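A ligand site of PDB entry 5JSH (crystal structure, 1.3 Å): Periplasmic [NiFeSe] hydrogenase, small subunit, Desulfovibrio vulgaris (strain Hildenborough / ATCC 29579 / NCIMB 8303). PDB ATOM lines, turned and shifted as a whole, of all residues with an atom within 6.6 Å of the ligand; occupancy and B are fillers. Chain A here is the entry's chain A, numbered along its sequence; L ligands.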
ATOM      1  N   ILE A 241     -29.852 -20.934  -5.183  1.00  0.00           N
ATOM      2  CA  ILE A 241     -28.703 -20.041  -5.154  1.00  0.00           C
ATOM      3  C   ILE A 241     -28.418 -19.549  -3.736  1.00  0.00           C
ATOM      4  O   ILE A 241     -27.295 -19.660  -3.233  1.00  0.00           O
ATOM      5  CB  ILE A 241     -28.904 -18.875  -6.127  1.00  0.00           C
ATOM      6  CG1 ILE A 241     -28.829 -19.373  -7.570  1.00  0.00           C
ATOM      7  CG2 ILE A 241     -27.874 -17.764  -5.875  1.00  0.00           C
ATOM      8  CD1 ILE A 241     -28.946 -18.295  -8.600  1.00  0.00           C
ATOM      9  N   HIS A 242     -29.428 -18.963  -3.090  1.00  0.00           N
ATOM     10  CA  HIS A 242     -29.246 -18.301  -1.801  1.00  0.00           C
ATOM     11  C   HIS A 242     -28.729 -19.267  -0.737  1.00  0.00           C
ATOM     12  O   HIS A 242     -27.831 -18.914   0.045  1.00  0.00           O
ATOM     13  CB  HIS A 242     -30.589 -17.695  -1.409  1.00  0.00           C
ATOM     14  CG  HIS A 242     -30.643 -17.118  -0.031  1.00  0.00           C
ATOM     15  ND1 HIS A 242     -30.128 -15.873   0.288  1.00  0.00           N
ATOM     16  CD2 HIS A 242     -31.191 -17.599   1.103  1.00  0.00           C
ATOM     17  CE1 HIS A 242     -30.350 -15.631   1.565  1.00  0.00           C
ATOM     18  NE2 HIS A 242     -30.991 -16.668   2.076  1.00  0.00           N
ATOM     19  N   GLU A 243     -29.274 -20.479  -0.687  1.00  0.00           N
ATOM     20  CA  GLU A 243     -28.846 -21.412   0.353  1.00  0.00           C
ATOM     21  C   GLU A 243     -27.404 -21.857   0.171  1.00  0.00           C
ATOM     22  O   GLU A 243     -26.814 -22.399   1.116  1.00  0.00           O
ATOM     23  CB  GLU A 243     -29.773 -22.644   0.405  1.00  0.00           C
ATOM     24  CG  GLU A 243     -31.225 -22.332   0.740  1.00  0.00           C
ATOM     25  CD  GLU A 243     -31.409 -21.557   2.026  1.00  0.00           C
ATOM     26  OE1 GLU A 243     -30.642 -21.764   2.994  1.00  0.00           O
ATOM     27  OE2 GLU A 243     -32.334 -20.735   2.096  1.00  0.00           O
ATOM     28  N   CYS A 245     -25.075 -19.514  -1.185  1.00  0.00           N
ATOM     29  CA  CYS A 245     -24.407 -18.277  -1.586  1.00  0.00           C
ATOM     30  C   CYS A 245     -23.261 -17.940  -0.616  1.00  0.00           C
ATOM     31  O   CYS A 245     -23.412 -18.085   0.601  1.00  0.00           O
ATOM     32  CB  CYS A 245     -25.406 -17.132  -1.592  1.00  0.00           C
ATOM     33  SG  CYS A 245     -24.682 -15.538  -2.065  1.00  0.00           S
ATOM     34  N   PRO A 246     -22.114 -17.477  -1.126  1.00  0.00           N
ATOM     35  CA  PRO A 246     -21.025 -17.066  -0.228  1.00  0.00           C
ATOM     36  C   PRO A 246     -21.358 -15.877   0.673  1.00  0.00           C
ATOM     37  O   PRO A 246     -20.625 -15.647   1.634  1.00  0.00           O
ATOM     38  CB  PRO A 246     -19.880 -16.727  -1.193  1.00  0.00           C
ATOM     39  CG  PRO A 246     -20.539 -16.426  -2.465  1.00  0.00           C
ATOM     40  CD  PRO A 246     -21.763 -17.291  -2.545  1.00  0.00           C
ATOM     41  N   TYR A 247     -22.437 -15.129   0.400  1.00  0.00           N
ATOM     42  CA  TYR A 247     -22.812 -13.994   1.230  1.00  0.00           C
ATOM     43  C   TYR A 247     -23.937 -14.326   2.203  1.00  0.00           C
ATOM     44  O   TYR A 247     -24.456 -13.431   2.861  1.00  0.00           O
ATOM     45  CB  TYR A 247     -23.165 -12.780   0.347  1.00  0.00           C
ATOM     46  CG  TYR A 247     -22.120 -12.614  -0.746  1.00  0.00           C
ATOM     47  CD1 TYR A 247     -20.808 -12.345  -0.422  1.00  0.00           C
ATOM     48  CD2 TYR A 247     -22.450 -12.785  -2.086  1.00  0.00           C
ATOM     49  CE1 TYR A 247     -19.829 -12.218  -1.395  1.00  0.00           C
ATOM     50  CE2 TYR A 247     -21.477 -12.668  -3.072  1.00  0.00           C
ATOM     51  CZ  TYR A 247     -20.172 -12.386  -2.731  1.00  0.00           C
ATOM     52  OH  TYR A 247     -19.231 -12.276  -3.745  1.00  0.00           O
ATOM     53  N   LEU A 248     -24.281 -15.620   2.335  1.00  0.00           N
ATOM     54  CA  LEU A 248     -25.407 -16.041   3.174  1.00  0.00           C
ATOM     55  C   LEU A 248     -25.224 -15.609   4.626  1.00  0.00           C
ATOM     56  O   LEU A 248     -26.192 -15.274   5.313  1.00  0.00           O
ATOM     57  CB  LEU A 248     -25.573 -17.557   3.059  1.00  0.00           C
ATOM     58  CG  LEU A 248     -26.752 -18.170   3.817  1.00  0.00           C
ATOM     59  CD1 LEU A 248     -28.086 -17.549   3.421  1.00  0.00           C
ATOM     60  CD2 LEU A 248     -26.761 -19.683   3.616  1.00  0.00           C
ATOM     61  N   ASP A 249     -23.993 -15.647   5.129  1.00  0.00           N
ATOM     62  CA  ASP A 249     -23.763 -15.203   6.501  1.00  0.00           C
ATOM     63  C   ASP A 249     -24.095 -13.721   6.670  1.00  0.00           C
ATOM     64  O   ASP A 249     -24.661 -13.319   7.697  1.00  0.00           O
ATOM     65  CB  ASP A 249     -22.318 -15.476   6.917  1.00  0.00           C
ATOM     66  CG  ASP A 249     -22.063 -16.956   7.183  1.00  0.00           C
ATOM     67  OD1 ASP A 249     -23.007 -17.768   7.091  1.00  0.00           O
ATOM     68  OD2 ASP A 249     -20.898 -17.293   7.468  1.00  0.00           O
ATOM     69  N   LYS A 250     -23.755 -12.892   5.678  1.00  0.00           N
ATOM     70  CA  LYS A 250     -24.107 -11.482   5.733  1.00  0.00           C
ATOM     71  C   LYS A 250     -25.621 -11.286   5.714  1.00  0.00           C
ATOM     72  O   LYS A 250     -26.159 -10.471   6.478  1.00  0.00           O
ATOM     73  CB  LYS A 250     -23.435 -10.739   4.578  1.00  0.00           C
ATOM     74  CG  LYS A 250     -21.914 -10.847   4.602  1.00  0.00           C
ATOM     75  CD  LYS A 250     -21.331 -10.180   5.860  1.00  0.00           C
ATOM     76  CE  LYS A 250     -19.826 -10.223   5.853  1.00  0.00           C
ATOM     77  NZ  LYS A 250     -19.262  -9.529   7.027  1.00  0.00           N
ATOM     78  N   TYR A 251     -26.327 -12.054   4.868  1.00  0.00           N
ATOM     79  CA  TYR A 251     -27.787 -12.010   4.876  1.00  0.00           C
ATOM     80  C   TYR A 251     -28.340 -12.307   6.260  1.00  0.00           C
ATOM     81  O   TYR A 251     -29.157 -11.564   6.796  1.00  0.00           O
ATOM     82  CB  TYR A 251     -28.347 -13.001   3.855  1.00  0.00           C
ATOM     83  CG  TYR A 251     -29.856 -13.112   3.846  1.00  0.00           C
ATOM     84  CD1 TYR A 251     -30.503 -14.020   4.676  1.00  0.00           C
ATOM     85  CD2 TYR A 251     -30.623 -12.340   2.990  1.00  0.00           C
ATOM     86  CE1 TYR A 251     -31.869 -14.137   4.667  1.00  0.00           C
ATOM     87  CE2 TYR A 251     -31.991 -12.454   2.971  1.00  0.00           C
ATOM     88  CZ  TYR A 251     -32.616 -13.360   3.797  1.00  0.00           C
ATOM     89  OH  TYR A 251     -33.987 -13.469   3.792  1.00  0.00           O
ATOM     90  N   ASP A 252     -27.878 -13.408   6.856  1.00  0.00           N
ATOM     91  CA  ASP A 252     -28.402 -13.820   8.145  1.00  0.00           C
ATOM     92  C   ASP A 252     -28.060 -12.827   9.246  1.00  0.00           C
ATOM     93  O   ASP A 252     -28.810 -12.712  10.213  1.00  0.00           O
ATOM     94  CB  ASP A 252     -27.919 -15.233   8.468  1.00  0.00           C
ATOM     95  CG  ASP A 252     -28.593 -16.297   7.609  1.00  0.00           C
ATOM     96  OD1 ASP A 252     -29.721 -16.076   7.129  1.00  0.00           O
ATOM     97  OD2 ASP A 252     -27.995 -17.382   7.409  1.00  0.00           O
ATOM     98  N   MET A 256     -26.194  -5.564   4.815  1.00  0.00           N
ATOM     99  CA  MET A 256     -26.644  -5.371   3.443  1.00  0.00           C
ATOM    100  C   MET A 256     -25.869  -4.254   2.778  1.00  0.00           C
ATOM    101  O   MET A 256     -25.769  -3.157   3.322  1.00  0.00           O
ATOM    102  CB  MET A 256     -28.117  -4.964   3.417  1.00  0.00           C
ATOM    103  CG  MET A 256     -29.023  -6.000   4.006  1.00  0.00           C
ATOM    104  SD  MET A 256     -29.048  -7.437   2.955  1.00  0.00           S
ATOM    105  CE  MET A 256     -30.024  -8.523   3.994  1.00  0.00           C
ATOM    106  N   GLY A 265     -21.166  -6.866   1.733  1.00  0.00           N
ATOM    107  CA  GLY A 265     -22.495  -7.156   2.229  1.00  0.00           C
ATOM    108  C   GLY A 265     -23.311  -8.041   1.285  1.00  0.00           C
ATOM    109  O   GLY A 265     -22.969  -8.282   0.131  1.00  0.00           O
ATOM    110  N   CYS A 266     -24.439  -8.516   1.819  1.00  0.00           N
ATOM    111  CA  CYS A 266     -25.411  -9.224   0.996  1.00  0.00           C
ATOM    112  C   CYS A 266     -26.097  -8.216   0.067  1.00  0.00           C
ATOM    113  O   CYS A 266     -26.192  -7.016   0.375  1.00  0.00           O
ATOM    114  CB  CYS A 266     -26.417  -9.924   1.925  1.00  0.00           C
ATOM    115  SG  CYS A 266     -27.990 -10.487   1.202  1.00  0.00           S
ATOM    116  N   ARG A 267     -26.552  -8.719  -1.093  1.00  0.00           N
ATOM    117  CA  ARG A 267     -27.159  -7.937  -2.162  1.00  0.00           C
ATOM    118  C   ARG A 267     -28.690  -7.885  -2.094  1.00  0.00           C
ATOM    119  O   ARG A 267     -29.320  -7.332  -3.005  1.00  0.00           O
ATOM    120  CB  ARG A 267     -26.696  -8.500  -3.517  1.00  0.00           C
ATOM    121  CG  ARG A 267     -25.240  -8.223  -3.905  1.00  0.00           C
ATOM    122  CD  ARG A 267     -24.189  -8.947  -3.073  1.00  0.00           C
ATOM    123  NE  ARG A 267     -22.964  -9.074  -3.848  1.00  0.00           N
ATOM    124  CZ  ARG A 267     -21.736  -9.128  -3.370  1.00  0.00           C
ATOM    125  NH1 ARG A 267     -21.487  -9.038  -2.059  1.00  0.00           N
ATOM    126  NH2 ARG A 267     -20.717  -9.221  -4.207  1.00  0.00           N
ATOM    127  N   TYR A 268     -29.294  -8.413  -1.037  1.00  0.00           N
ATOM    128  CA  TYR A 268     -30.751  -8.509  -0.956  1.00  0.00           C
ATOM    129  C   TYR A 268     -31.443  -7.145  -1.099  1.00  0.00           C
ATOM    130  O   TYR A 268     -32.437  -7.011  -1.827  1.00  0.00           O
ATOM    131  CB  TYR A 268     -31.131  -9.190   0.347  1.00  0.00           C
ATOM    132  CG  TYR A 268     -32.613  -9.354   0.552  1.00  0.00           C
ATOM    133  CD1 TYR A 268     -33.300 -10.381  -0.069  1.00  0.00           C
ATOM    134  CD2 TYR A 268     -33.310  -8.500   1.384  1.00  0.00           C
ATOM    135  CE1 TYR A 268     -34.646 -10.561   0.123  1.00  0.00           C
ATOM    136  CE2 TYR A 268     -34.665  -8.663   1.583  1.00  0.00           C
ATOM    137  CZ  TYR A 268     -35.319  -9.689   0.945  1.00  0.00           C
ATOM    138  OH  TYR A 268     -36.666  -9.866   1.159  1.00  0.00           O
ATOM    139  N   ASP A 269     -30.976  -6.129  -0.371  1.00  0.00           N
ATOM    140  CA  ASP A 269     -31.647  -4.836  -0.434  1.00  0.00           C
ATOM    141  C   ASP A 269     -31.504  -4.188  -1.802  1.00  0.00           C
ATOM    142  O   ASP A 269     -32.329  -3.347  -2.186  1.00  0.00           O
ATOM    143  CB  ASP A 269     -31.098  -3.883   0.632  1.00  0.00           C
ATOM    144  CG  ASP A 269     -31.606  -4.177   2.040  1.00  0.00           C
ATOM    145  OD1 ASP A 269     -32.483  -5.047   2.226  1.00  0.00           O
ATOM    146  OD2 ASP A 269     -31.120  -3.503   2.957  1.00  0.00           O
ATOM    147  N   CYS A 272     -31.409  -8.561  -5.043  1.00  0.00           N
ATOM    148  CA  CYS A 272     -31.042  -9.932  -5.366  1.00  0.00           C
ATOM    149  C   CYS A 272     -32.223 -10.897  -5.187  1.00  0.00           C
ATOM    150  O   CYS A 272     -32.843 -10.959  -4.121  1.00  0.00           O
ATOM    151  CB  CYS A 272     -29.886 -10.356  -4.465  1.00  0.00           C
ATOM    152  SG  CYS A 272     -29.203 -12.002  -4.931  1.00  0.00           S
ATOM    153  N   LYS A 273     -32.470 -11.710  -6.210  1.00  0.00           N
ATOM    154  CA  LYS A 273     -33.519 -12.733  -6.206  1.00  0.00           C
ATOM    155  C   LYS A 273     -32.999 -14.133  -5.951  1.00  0.00           C
ATOM    156  O   LYS A 273     -33.734 -15.112  -6.150  1.00  0.00           O
ATOM    157  CB  LYS A 273     -34.341 -12.690  -7.490  1.00  0.00           C
ATOM    158  CG  LYS A 273     -34.921 -11.290  -7.796  1.00  0.00           C
ATOM    159  CD  LYS A 273     -35.701 -10.728  -6.598  1.00  0.00           C
ATOM    160  CE  LYS A 273     -36.521  -9.475  -6.961  1.00  0.00           C
ATOM    161  NZ  LYS A 273     -35.683  -8.446  -7.592  1.00  0.00           N
ATOM    162  N   GLY A 274     -31.745 -14.275  -5.517  1.00  0.00           N
ATOM    163  CA  GLY A 274     -31.198 -15.555  -5.135  1.00  0.00           C
ATOM    164  C   GLY A 274     -32.114 -16.437  -4.292  1.00  0.00           C
ATOM    165  O   GLY A 274     -32.192 -17.653  -4.504  1.00  0.00           O
ATOM    166  N   PRO A 275     -32.805 -15.842  -3.306  1.00  0.00           N
ATOM    167  CA  PRO A 275     -33.666 -16.678  -2.439  1.00  0.00           C
ATOM    168  C   PRO A 275     -34.724 -17.472  -3.174  1.00  0.00           C
ATOM    169  O   PRO A 275     -35.135 -18.529  -2.687  1.00  0.00           O
ATOM    170  CB  PRO A 275     -34.263 -15.649  -1.456  1.00  0.00           C
ATOM    171  CG  PRO A 275     -33.243 -14.570  -1.372  1.00  0.00           C
ATOM    172  CD  PRO A 275     -32.674 -14.481  -2.793  1.00  0.00           C
ATOM    173  N   TRP A 292     -19.911 -13.950 -11.795  1.00  0.00           N
ATOM    174  CA  TRP A 292     -21.306 -14.338 -11.840  1.00  0.00           C
ATOM    175  C   TRP A 292     -22.158 -13.195 -11.311  1.00  0.00           C
ATOM    176  O   TRP A 292     -21.642 -12.216 -10.744  1.00  0.00           O
ATOM    177  CB  TRP A 292     -21.597 -15.647 -11.093  1.00  0.00           C
ATOM    178  CG  TRP A 292     -21.451 -15.628  -9.612  1.00  0.00           C
ATOM    179  CD1 TRP A 292     -20.329 -15.324  -8.882  1.00  0.00           C
ATOM    180  CD2 TRP A 292     -22.449 -16.003  -8.657  1.00  0.00           C
ATOM    181  NE1 TRP A 292     -20.576 -15.494  -7.534  1.00  0.00           N
ATOM    182  CE2 TRP A 292     -21.876 -15.894  -7.368  1.00  0.00           C
ATOM    183  CE3 TRP A 292     -23.779 -16.427  -8.759  1.00  0.00           C
ATOM    184  CZ2 TRP A 292     -22.568 -16.207  -6.215  1.00  0.00           C
ATOM    185  CZ3 TRP A 292     -24.473 -16.716  -7.608  1.00  0.00           C
ATOM    186  CH2 TRP A 292     -23.870 -16.602  -6.346  1.00  0.00           C
ATOM    187  N   VAL A 294     -24.297 -12.528  -8.889  1.00  0.00           N
ATOM    188  CA  VAL A 294     -24.342 -12.087  -7.502  1.00  0.00           C
ATOM    189  C   VAL A 294     -23.045 -11.387  -7.115  1.00  0.00           C
ATOM    190  O   VAL A 294     -23.059 -10.382  -6.393  1.00  0.00           O
ATOM    191  CB  VAL A 294     -24.678 -13.265  -6.577  1.00  0.00           C
ATOM    192  CG1 VAL A 294     -24.565 -12.852  -5.115  1.00  0.00           C
ATOM    193  CG2 VAL A 294     -26.062 -13.768  -6.852  1.00  0.00           C
ATOM    194  N   ALA A 297     -23.276  -7.894  -9.337  1.00  0.00           N
ATOM    195  CA  ALA A 297     -24.428  -7.032  -9.173  1.00  0.00           C
ATOM    196  C   ALA A 297     -25.486  -7.771  -8.362  1.00  0.00           C
ATOM    197  O   ALA A 297     -25.297  -7.964  -7.159  1.00  0.00           O
ATOM    198  CB  ALA A 297     -24.961  -6.574 -10.530  1.00  0.00           C
ATOM    199  N   CYS A 299     -28.588 -11.215  -8.646  1.00  0.00           N
ATOM    200  CA  CYS A 299     -29.353 -12.215  -9.402  1.00  0.00           C
ATOM    201  C   CYS A 299     -30.736 -11.663  -9.702  1.00  0.00           C
ATOM    202  O   CYS A 299     -31.403 -11.078  -8.831  1.00  0.00           O
ATOM    203  CB  CYS A 299     -29.460 -13.519  -8.597  1.00  0.00           C
ATOM    204  SG  CYS A 299     -30.482 -14.833  -9.331  1.00  0.00           S
HETATM  205 FE1  LIG L   1     -28.485 -12.797  -2.895  1.00  0.00          FE
HETATM  206 FE2  LIG L   1     -29.031 -14.521  -0.812  1.00  0.00          FE
HETATM  207 FE3  LIG L   1     -27.721 -12.218  -0.260  1.00  0.00          FE
HETATM  208 FE4  LIG L   1     -26.521 -14.235  -1.660  1.00  0.00          FE
HETATM  209  S1  LIG L   1     -27.163 -14.270   0.532  1.00  0.00           S
HETATM  210  S2  LIG L   1     -26.411 -11.999  -2.121  1.00  0.00           S
HETATM  211  S3  LIG L   1     -28.277 -15.092  -2.905  1.00  0.00           S
HETATM  212  S4  LIG L   1     -29.877 -12.402  -1.114  1.00  0.00           S
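An iron atom (FE2) of the ligand is bound by a ring nitrogen (ND1) of His 242, 2.1 Å away.
The side-chain sulfur of Cys 266 is bound to an iron atom (FE3) of the ligand.
FE4 of the ligand is bound by SG of Cys 245, 2.3 Å away.
The side-chain sulfur (SG) of Cys 272 is bound to an iron atom (FE1) of the ligand (2.3 Å).
N of Arg 267 lies close to S2 of the ligand (3.4 Å).
N of Leu 248 sits close to S1 of the ligand (3.7 Å).
The backbone carbonyl oxygen of Gly 274 sits at hydrogen-bond distance from the backbone NH of His 242.
The side-chain sulfur of Cys 266 lies close to the backbone NH of Tyr 268, at 3.3 Å.
The side-chain sulfur (SG) of Cys 245 sits close to the backbone NH (N) of Tyr 247 (3.4 Å).
The backbone carbonyl oxygen (O) of Arg 267 lies within hydrogen-bond range of the backbone NH (N) of Cys 272 (3.2 Å).
N of Gly 274 sits close to SG of Cys 272 (3.5 Å).
NE of Arg 267 is in hydrogen-bond range of O of Val 294 (2.9 Å).
OH of Tyr 247 sits at hydrogen-bond distance from NH2 of Arg 267, at 3.4 Å.
The guanidinium group (NH1) of Arg 267 lies within hydrogen-bond range of the backbone carbonyl oxygen (O) of Gly 265.
O of Tyr 247 sits close to S1 of the ligand (3.7 Å).
Merely in contact with the ligand: Tyr 251 (3.7 Å), Tyr 268 (3.7 Å), Gly 274 (3.7 Å), Pro 275 (3.9 Å) and Val 294 (3.6 Å).
Hydrophobic or aromatic side chains within 4 Å of the ligand: His 242, Tyr 251, Tyr 268, Pro 275 and Val 294.
12 residues have an atom within 4 Å of the ligand: His 242, Cys 245, Tyr 247, Leu 248, Tyr 251, Cys 266, Arg 267, Tyr 268, Cys 272, Gly 274, Pro 275 and Val 294.
The nearest printed residue that does not touch the ligand is Ile 241 (4.02 Å).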
